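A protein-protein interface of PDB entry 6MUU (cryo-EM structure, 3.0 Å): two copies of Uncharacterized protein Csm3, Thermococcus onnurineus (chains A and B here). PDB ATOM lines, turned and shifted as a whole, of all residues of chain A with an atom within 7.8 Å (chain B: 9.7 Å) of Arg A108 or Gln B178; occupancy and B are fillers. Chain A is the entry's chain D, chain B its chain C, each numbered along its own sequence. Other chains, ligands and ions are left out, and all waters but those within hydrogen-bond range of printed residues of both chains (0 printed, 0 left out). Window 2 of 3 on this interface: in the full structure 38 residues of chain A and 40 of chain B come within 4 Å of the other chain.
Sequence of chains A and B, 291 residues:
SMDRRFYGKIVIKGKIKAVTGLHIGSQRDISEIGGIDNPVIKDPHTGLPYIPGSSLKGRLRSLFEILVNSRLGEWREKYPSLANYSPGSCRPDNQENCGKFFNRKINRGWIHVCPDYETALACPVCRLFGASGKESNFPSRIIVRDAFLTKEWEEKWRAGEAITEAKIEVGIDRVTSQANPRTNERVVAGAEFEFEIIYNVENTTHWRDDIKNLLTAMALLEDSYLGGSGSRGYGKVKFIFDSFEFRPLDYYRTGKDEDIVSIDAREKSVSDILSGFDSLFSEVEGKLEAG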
ATOM      1  N   ARG A  91       9.545 -14.802   0.313  1.00  0.00           N
ATOM      2  CA  ARG A  91      10.544 -13.755   0.510  1.00  0.00           C
ATOM      3  C   ARG A  91      10.756 -12.845  -0.709  1.00  0.00           C
ATOM      4  O   ARG A  91      10.813 -11.624  -0.510  1.00  0.00           O
ATOM      5  CB  ARG A  91      11.872 -14.383   0.965  1.00  0.00           C
ATOM      6  CG  ARG A  91      13.013 -13.402   1.214  1.00  0.00           C
ATOM      7  CD  ARG A  91      12.757 -12.552   2.437  1.00  0.00           C
ATOM      8  NE  ARG A  91      13.893 -11.693   2.745  1.00  0.00           N
ATOM      9  CZ  ARG A  91      13.898 -10.787   3.716  1.00  0.00           C
ATOM     10  NH1 ARG A  91      14.977 -10.045   3.928  1.00  0.00           N
ATOM     11  NH2 ARG A  91      12.830 -10.630   4.485  1.00  0.00           N
ATOM     12  N   ASN A  94       6.817  -9.908  -2.127  1.00  0.00           N
ATOM     13  CA  ASN A  94       6.378  -9.483  -0.797  1.00  0.00           C
ATOM     14  C   ASN A  94       4.854  -9.533  -0.727  1.00  0.00           C
ATOM     15  O   ASN A  94       4.158  -8.519  -0.805  1.00  0.00           O
ATOM     16  CB  ASN A  94       6.899  -8.087  -0.484  1.00  0.00           C
ATOM     17  CG  ASN A  94       8.403  -8.048  -0.324  1.00  0.00           C
ATOM     18  OD1 ASN A  94       8.999  -8.948   0.263  1.00  0.00           O
ATOM     19  ND2 ASN A  94       9.026  -7.000  -0.843  1.00  0.00           N
ATOM     20  N   ARG A 104       3.367 -16.220   5.911  1.00  0.00           N
ATOM     21  CA  ARG A 104       3.161 -15.039   6.740  1.00  0.00           C
ATOM     22  C   ARG A 104       4.497 -14.480   7.187  1.00  0.00           C
ATOM     23  O   ARG A 104       5.338 -15.220   7.700  1.00  0.00           O
ATOM     24  CB  ARG A 104       2.311 -15.349   7.972  1.00  0.00           C
ATOM     25  CG  ARG A 104       1.924 -14.107   8.761  1.00  0.00           C
ATOM     26  CD  ARG A 104       1.110 -14.452   9.983  1.00  0.00           C
ATOM     27  NE  ARG A 104      -0.129 -15.129   9.624  1.00  0.00           N
ATOM     28  CZ  ARG A 104      -1.266 -14.526   9.307  1.00  0.00           C
ATOM     29  NH1 ARG A 104      -1.348 -13.205   9.301  1.00  0.00           N
ATOM     30  NH2 ARG A 104      -2.324 -15.255   8.996  1.00  0.00           N
ATOM     31  N   LYS A 105       4.689 -13.181   6.996  1.00  0.00           N
ATOM     32  CA  LYS A 105       5.839 -12.503   7.560  1.00  0.00           C
ATOM     33  C   LYS A 105       5.477 -11.975   8.935  1.00  0.00           C
ATOM     34  O   LYS A 105       4.322 -11.628   9.198  1.00  0.00           O
ATOM     35  CB  LYS A 105       6.324 -11.363   6.660  1.00  0.00           C
ATOM     36  CG  LYS A 105       5.381 -10.192   6.516  1.00  0.00           C
ATOM     37  CD  LYS A 105       5.918  -9.161   5.544  1.00  0.00           C
ATOM     38  CE  LYS A 105       7.092  -8.415   6.139  1.00  0.00           C
ATOM     39  NZ  LYS A 105       7.544  -7.308   5.261  1.00  0.00           N
ATOM     40  N   ILE A 106       6.458 -11.960   9.827  1.00  0.00           N
ATOM     41  CA  ILE A 106       6.218 -11.479  11.178  1.00  0.00           C
ATOM     42  C   ILE A 106       6.555 -10.001  11.243  1.00  0.00           C
ATOM     43  O   ILE A 106       5.670  -9.158  11.422  1.00  0.00           O
ATOM     44  CB  ILE A 106       7.039 -12.289  12.190  1.00  0.00           C
ATOM     45  CG1 ILE A 106       6.626 -13.752  12.118  1.00  0.00           C
ATOM     46  CG2 ILE A 106       6.848 -11.750  13.586  1.00  0.00           C
ATOM     47  CD1 ILE A 106       5.177 -13.991  12.454  1.00  0.00           C
ATOM     48  N   ASN A 107       7.831  -9.676  11.089  1.00  0.00           N
ATOM     49  CA  ASN A 107       8.262  -8.300  10.901  1.00  0.00           C
ATOM     50  C   ASN A 107       9.078  -8.152   9.632  1.00  0.00           C
ATOM     51  O   ASN A 107       8.818  -7.252   8.826  1.00  0.00           O
ATOM     52  CB  ASN A 107       9.064  -7.840  12.128  1.00  0.00           C
ATOM     53  CG  ASN A 107       9.224  -6.336  12.200  1.00  0.00           C
ATOM     54  OD1 ASN A 107       8.775  -5.601  11.321  1.00  0.00           O
ATOM     55  ND2 ASN A 107       9.853  -5.869  13.270  1.00  0.00           N
ATOM     56  N   ARG A 108      10.067  -9.020   9.442  1.00  0.00           N
ATOM     57  CA  ARG A 108      10.842  -9.086   8.218  1.00  0.00           C
ATOM     58  C   ARG A 108      11.013 -10.508   7.716  1.00  0.00           C
ATOM     59  O   ARG A 108      11.431 -10.687   6.568  1.00  0.00           O
ATOM     60  CB  ARG A 108      12.239  -8.471   8.410  1.00  0.00           C
ATOM     61  CG  ARG A 108      12.320  -6.945   8.359  1.00  0.00           C
ATOM     62  CD  ARG A 108      11.993  -6.289   9.694  1.00  0.00           C
ATOM     63  NE  ARG A 108      12.109  -4.835   9.645  1.00  0.00           N
ATOM     64  CZ  ARG A 108      13.237  -4.166   9.860  1.00  0.00           C
ATOM     65  NH1 ARG A 108      14.357  -4.822  10.136  1.00  0.00           N
ATOM     66  NH2 ARG A 108      13.247  -2.842   9.797  1.00  0.00           N
ATOM     67  N   GLY A 109      10.708 -11.515   8.527  1.00  0.00           N
ATOM     68  CA  GLY A 109      10.972 -12.895   8.176  1.00  0.00           C
ATOM     69  C   GLY A 109       9.692 -13.694   8.051  1.00  0.00           C
ATOM     70  O   GLY A 109       8.725 -13.456   8.772  1.00  0.00           O
ATOM     71  N   TRP A 110       9.712 -14.673   7.150  1.00  0.00           N
ATOM     72  CA  TRP A 110       8.522 -15.392   6.715  1.00  0.00           C
ATOM     73  C   TRP A 110       8.451 -16.734   7.428  1.00  0.00           C
ATOM     74  O   TRP A 110       9.407 -17.513   7.389  1.00  0.00           O
ATOM     75  CB  TRP A 110       8.554 -15.574   5.198  1.00  0.00           C
ATOM     76  CG  TRP A 110       8.566 -14.256   4.499  1.00  0.00           C
ATOM     77  CD1 TRP A 110       9.663 -13.510   4.188  1.00  0.00           C
ATOM     78  CD2 TRP A 110       7.438 -13.527   4.013  1.00  0.00           C
ATOM     79  NE1 TRP A 110       9.287 -12.352   3.561  1.00  0.00           N
ATOM     80  CE2 TRP A 110       7.924 -12.342   3.434  1.00  0.00           C
ATOM     81  CE3 TRP A 110       6.068 -13.760   4.008  1.00  0.00           C
ATOM     82  CZ2 TRP A 110       7.087 -11.395   2.862  1.00  0.00           C
ATOM     83  CZ3 TRP A 110       5.240 -12.814   3.439  1.00  0.00           C
ATOM     84  CH2 TRP A 110       5.750 -11.651   2.875  1.00  0.00           C
ATOM     85  N   ILE A 111       7.324 -16.986   8.090  1.00  0.00           N
ATOM     86  CA  ILE A 111       7.073 -18.197   8.858  1.00  0.00           C
ATOM     87  C   ILE A 111       5.767 -18.789   8.356  1.00  0.00           C
ATOM     88  O   ILE A 111       4.826 -18.046   8.060  1.00  0.00           O
ATOM     89  CB  ILE A 111       7.000 -17.882  10.369  1.00  0.00           C
ATOM     90  CG1 ILE A 111       8.352 -17.388  10.868  1.00  0.00           C
ATOM     91  CG2 ILE A 111       6.554 -19.070  11.205  1.00  0.00           C
ATOM     92  CD1 ILE A 111       8.335 -16.951  12.297  1.00  0.00           C
ATOM     93  N   VAL B 170      11.971 -13.415  20.186  1.00  0.00           N
ATOM     94  CA  VAL B 170      12.382 -13.053  18.841  1.00  0.00           C
ATOM     95  C   VAL B 170      11.589 -13.928  17.869  1.00  0.00           C
ATOM     96  O   VAL B 170      10.946 -14.895  18.265  1.00  0.00           O
ATOM     97  CB  VAL B 170      13.905 -13.219  18.661  1.00  0.00           C
ATOM     98  CG1 VAL B 170      14.265 -14.642  18.393  1.00  0.00           C
ATOM     99  CG2 VAL B 170      14.473 -12.294  17.625  1.00  0.00           C
ATOM    100  N   GLY B 171      11.597 -13.549  16.594  1.00  0.00           N
ATOM    101  CA  GLY B 171      10.958 -14.359  15.574  1.00  0.00           C
ATOM    102  C   GLY B 171      11.887 -14.628  14.410  1.00  0.00           C
ATOM    103  O   GLY B 171      12.284 -13.700  13.705  1.00  0.00           O
ATOM    104  N   ILE B 172      12.235 -15.888  14.191  1.00  0.00           N
ATOM    105  CA  ILE B 172      13.296 -16.265  13.267  1.00  0.00           C
ATOM    106  C   ILE B 172      12.684 -16.690  11.940  1.00  0.00           C
ATOM    107  O   ILE B 172      11.741 -17.488  11.909  1.00  0.00           O
ATOM    108  CB  ILE B 172      14.164 -17.387  13.863  1.00  0.00           C
ATOM    109  CG1 ILE B 172      14.751 -16.936  15.192  1.00  0.00           C
ATOM    110  CG2 ILE B 172      15.300 -17.749  12.942  1.00  0.00           C
ATOM    111  CD1 ILE B 172      15.636 -15.740  15.077  1.00  0.00           C
ATOM    112  N   ASP B 173      13.210 -16.143  10.847  1.00  0.00           N
ATOM    113  CA  ASP B 173      12.879 -16.606   9.507  1.00  0.00           C
ATOM    114  C   ASP B 173      13.451 -18.001   9.281  1.00  0.00           C
ATOM    115  O   ASP B 173      14.523 -18.342   9.776  1.00  0.00           O
ATOM    116  CB  ASP B 173      13.438 -15.634   8.469  1.00  0.00           C
ATOM    117  CG  ASP B 173      13.018 -15.975   7.058  1.00  0.00           C
ATOM    118  OD1 ASP B 173      11.852 -15.720   6.703  1.00  0.00           O
ATOM    119  OD2 ASP B 173      13.854 -16.495   6.293  1.00  0.00           O
ATOM    120  N   ARG B 174      12.724 -18.816   8.520  1.00  0.00           N
ATOM    121  CA  ARG B 174      13.129 -20.210   8.365  1.00  0.00           C
ATOM    122  C   ARG B 174      14.148 -20.395   7.254  1.00  0.00           C
ATOM    123  O   ARG B 174      14.881 -21.389   7.250  1.00  0.00           O
ATOM    124  CB  ARG B 174      11.915 -21.097   8.101  1.00  0.00           C
ATOM    125  CG  ARG B 174      11.175 -21.500   9.347  1.00  0.00           C
ATOM    126  CD  ARG B 174      10.180 -20.460   9.771  1.00  0.00           C
ATOM    127  NE  ARG B 174       9.373 -20.940  10.879  1.00  0.00           N
ATOM    128  CZ  ARG B 174       9.631 -20.682  12.152  1.00  0.00           C
ATOM    129  NH1 ARG B 174       8.836 -21.168  13.088  1.00  0.00           N
ATOM    130  NH2 ARG B 174      10.669 -19.932  12.487  1.00  0.00           N
ATOM    131  N   VAL B 175      14.206 -19.467   6.310  1.00  0.00           N
ATOM    132  CA  VAL B 175      15.155 -19.562   5.212  1.00  0.00           C
ATOM    133  C   VAL B 175      16.421 -18.776   5.510  1.00  0.00           C
ATOM    134  O   VAL B 175      17.536 -19.268   5.324  1.00  0.00           O
ATOM    135  CB  VAL B 175      14.484 -19.081   3.908  1.00  0.00           C
ATOM    136  CG1 VAL B 175      15.454 -19.140   2.756  1.00  0.00           C
ATOM    137  CG2 VAL B 175      13.264 -19.910   3.608  1.00  0.00           C
ATOM    138  N   THR B 176      16.272 -17.550   5.999  1.00  0.00           N
ATOM    139  CA  THR B 176      17.391 -16.634   6.117  1.00  0.00           C
ATOM    140  C   THR B 176      17.889 -16.456   7.542  1.00  0.00           C
ATOM    141  O   THR B 176      18.962 -15.875   7.722  1.00  0.00           O
ATOM    142  CB  THR B 176      17.001 -15.268   5.553  1.00  0.00           C
ATOM    143  OG1 THR B 176      15.928 -14.726   6.327  1.00  0.00           O
ATOM    144  CG2 THR B 176      16.543 -15.410   4.119  1.00  0.00           C
ATOM    145  N   SER B 177      17.146 -16.950   8.538  1.00  0.00           N
ATOM    146  CA  SER B 177      17.396 -16.721   9.970  1.00  0.00           C
ATOM    147  C   SER B 177      17.426 -15.232  10.311  1.00  0.00           C
ATOM    148  O   SER B 177      18.234 -14.777  11.120  1.00  0.00           O
ATOM    149  CB  SER B 177      18.668 -17.422  10.460  1.00  0.00           C
ATOM    150  OG  SER B 177      19.827 -16.815   9.923  1.00  0.00           O
ATOM    151  N   GLN B 178      16.536 -14.470   9.686  1.00  0.00           N
ATOM    152  CA  GLN B 178      16.320 -13.082  10.070  1.00  0.00           C
ATOM    153  C   GLN B 178      15.609 -13.021  11.414  1.00  0.00           C
ATOM    154  O   GLN B 178      14.573 -13.661  11.603  1.00  0.00           O
ATOM    155  CB  GLN B 178      15.490 -12.369   9.006  1.00  0.00           C
ATOM    156  CG  GLN B 178      15.150 -10.930   9.335  1.00  0.00           C
ATOM    157  CD  GLN B 178      16.343 -10.017   9.263  1.00  0.00           C
ATOM    158  OE1 GLN B 178      17.137 -10.095   8.329  1.00  0.00           O
ATOM    159  NE2 GLN B 178      16.484  -9.147  10.252  1.00  0.00           N
ATOM    160  N   ALA B 179      16.152 -12.245  12.344  1.00  0.00           N
ATOM    161  CA  ALA B 179      15.620 -12.166  13.696  1.00  0.00           C
ATOM    162  C   ALA B 179      14.807 -10.895  13.890  1.00  0.00           C
ATOM    163  O   ALA B 179      15.200  -9.817  13.435  1.00  0.00           O
ATOM    164  CB  ALA B 179      16.748 -12.210  14.717  1.00  0.00           C
ATOM    165  N   ASN B 180      13.678 -11.024  14.585  1.00  0.00           N
ATOM    166  CA  ASN B 180      12.731  -9.926  14.782  1.00  0.00           C
ATOM    167  C   ASN B 180      12.286  -9.899  16.238  1.00  0.00           C
ATOM    168  O   ASN B 180      11.325 -10.581  16.614  1.00  0.00           O
ATOM    169  CB  ASN B 180      11.536 -10.082  13.851  1.00  0.00           C
ATOM    170  CG  ASN B 180      11.922  -9.959  12.402  1.00  0.00           C
ATOM    171  OD1 ASN B 180      12.700  -9.082  12.029  1.00  0.00           O
ATOM    172  ND2 ASN B 180      11.396 -10.849  11.573  1.00  0.00           N
ATOM    173  N   PRO B 181      12.956  -9.121  17.084  1.00  0.00           N
ATOM    174  CA  PRO B 181      12.689  -9.180  18.524  1.00  0.00           C
ATOM    175  C   PRO B 181      11.441  -8.419  18.945  1.00  0.00           C
ATOM    176  O   PRO B 181      10.919  -7.563  18.230  1.00  0.00           O
ATOM    177  CB  PRO B 181      13.942  -8.547  19.135  1.00  0.00           C
ATOM    178  CG  PRO B 181      14.453  -7.659  18.084  1.00  0.00           C
ATOM    179  CD  PRO B 181      14.150  -8.320  16.780  1.00  0.00           C
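The side-chain carboxylate (OD1) of Asp B173 is in hydrogen-bond range of the backbone NH (N) of Trp A110 (2.4 Å). The side-chain amide nitrogen of Asn B180 lies close to the backbone NH of Arg A108 (3.1 Å). ND2 of Asn B180 sits close to N of Gly A109, at 3.2 Å.
N of Gly B171 sits at hydrogen-bond distance from O of Asn B180, at 3.0 Å. The side-chain carboxylate (OD2) of Asp B173 is in hydrogen-bond range of the backbone NH (N) of Val B175, at 3.0 Å. OD2 of Asp B173 lies within hydrogen-bond range of N of Thr B176 (2.7 Å). The backbone NH (N) of Asp B173 sits at hydrogen-bond distance from the backbone carbonyl oxygen (O) of Gln B178, at 2.9 Å. The backbone carbonyl oxygen of Arg A108 lies within hydrogen-bond range of the guanidinium group of Arg A91 (2.5 Å). The backbone NH (N) of Ile A111 sits at hydrogen-bond distance from the backbone carbonyl oxygen (O) of Arg A104 (2.7 Å).
Among the printed residues, pairs that only touch across the chains: Gly A109 with Asp B173 (3.3 Å), Ile A111 with Arg B174 (3.4 Å), Ile A111 with Ile B172 (3.5 Å), Asn A107 with Asn B180 (3.6 Å), Trp A110 with Arg B174 (3.7 Å) and Arg A108 with Gln B178 (3.9 Å).
Arg A108 touches just these residues of chain B: Gln B178 (3.9 Å) and Asn B180 (3.1 Å). Printed residues of chain A within 4 Å of Gln B178: Arg A108. Asn A107 touches just one residue of chain B: Asn B180 (3.6 Å). Of the printed residues of chain A, Ile B172 touches Ile A111. Printed residues of chain A within 4 Å of Asp B173: Gly A109 and Trp A110. Printed residues of chain B within 4 Å of Ile A111: Ile B172 and Arg B174. Printed residues of chain A within 4 Å of Arg B174: Trp A110 (3.7 Å) and Ile A111 (3.4 Å). The nearest residue of chain A that does not touch Gln B178 is Gly A109 (4.6 Å). The nearest printed residue of chain B that does not touch Trp A110 is Ile B172 (5.1 Å).
Of the 12 printed residues of chain B, 5 touch a printed residue of chain A. Printed residues of chain A that touch a printed residue of chain B: Asn A107, Arg A108, Gly A109, Trp A110 and Ile A111. Among the printed residues, no Asp or Glu carboxylate lies within 4 Å of a Lys or Arg side-chain nitrogen of the other chain.
No position is printed for both chains. Of the 9 pairs that touch across the chains among the printed residues, none has its exchanged pair printed and touching as well.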
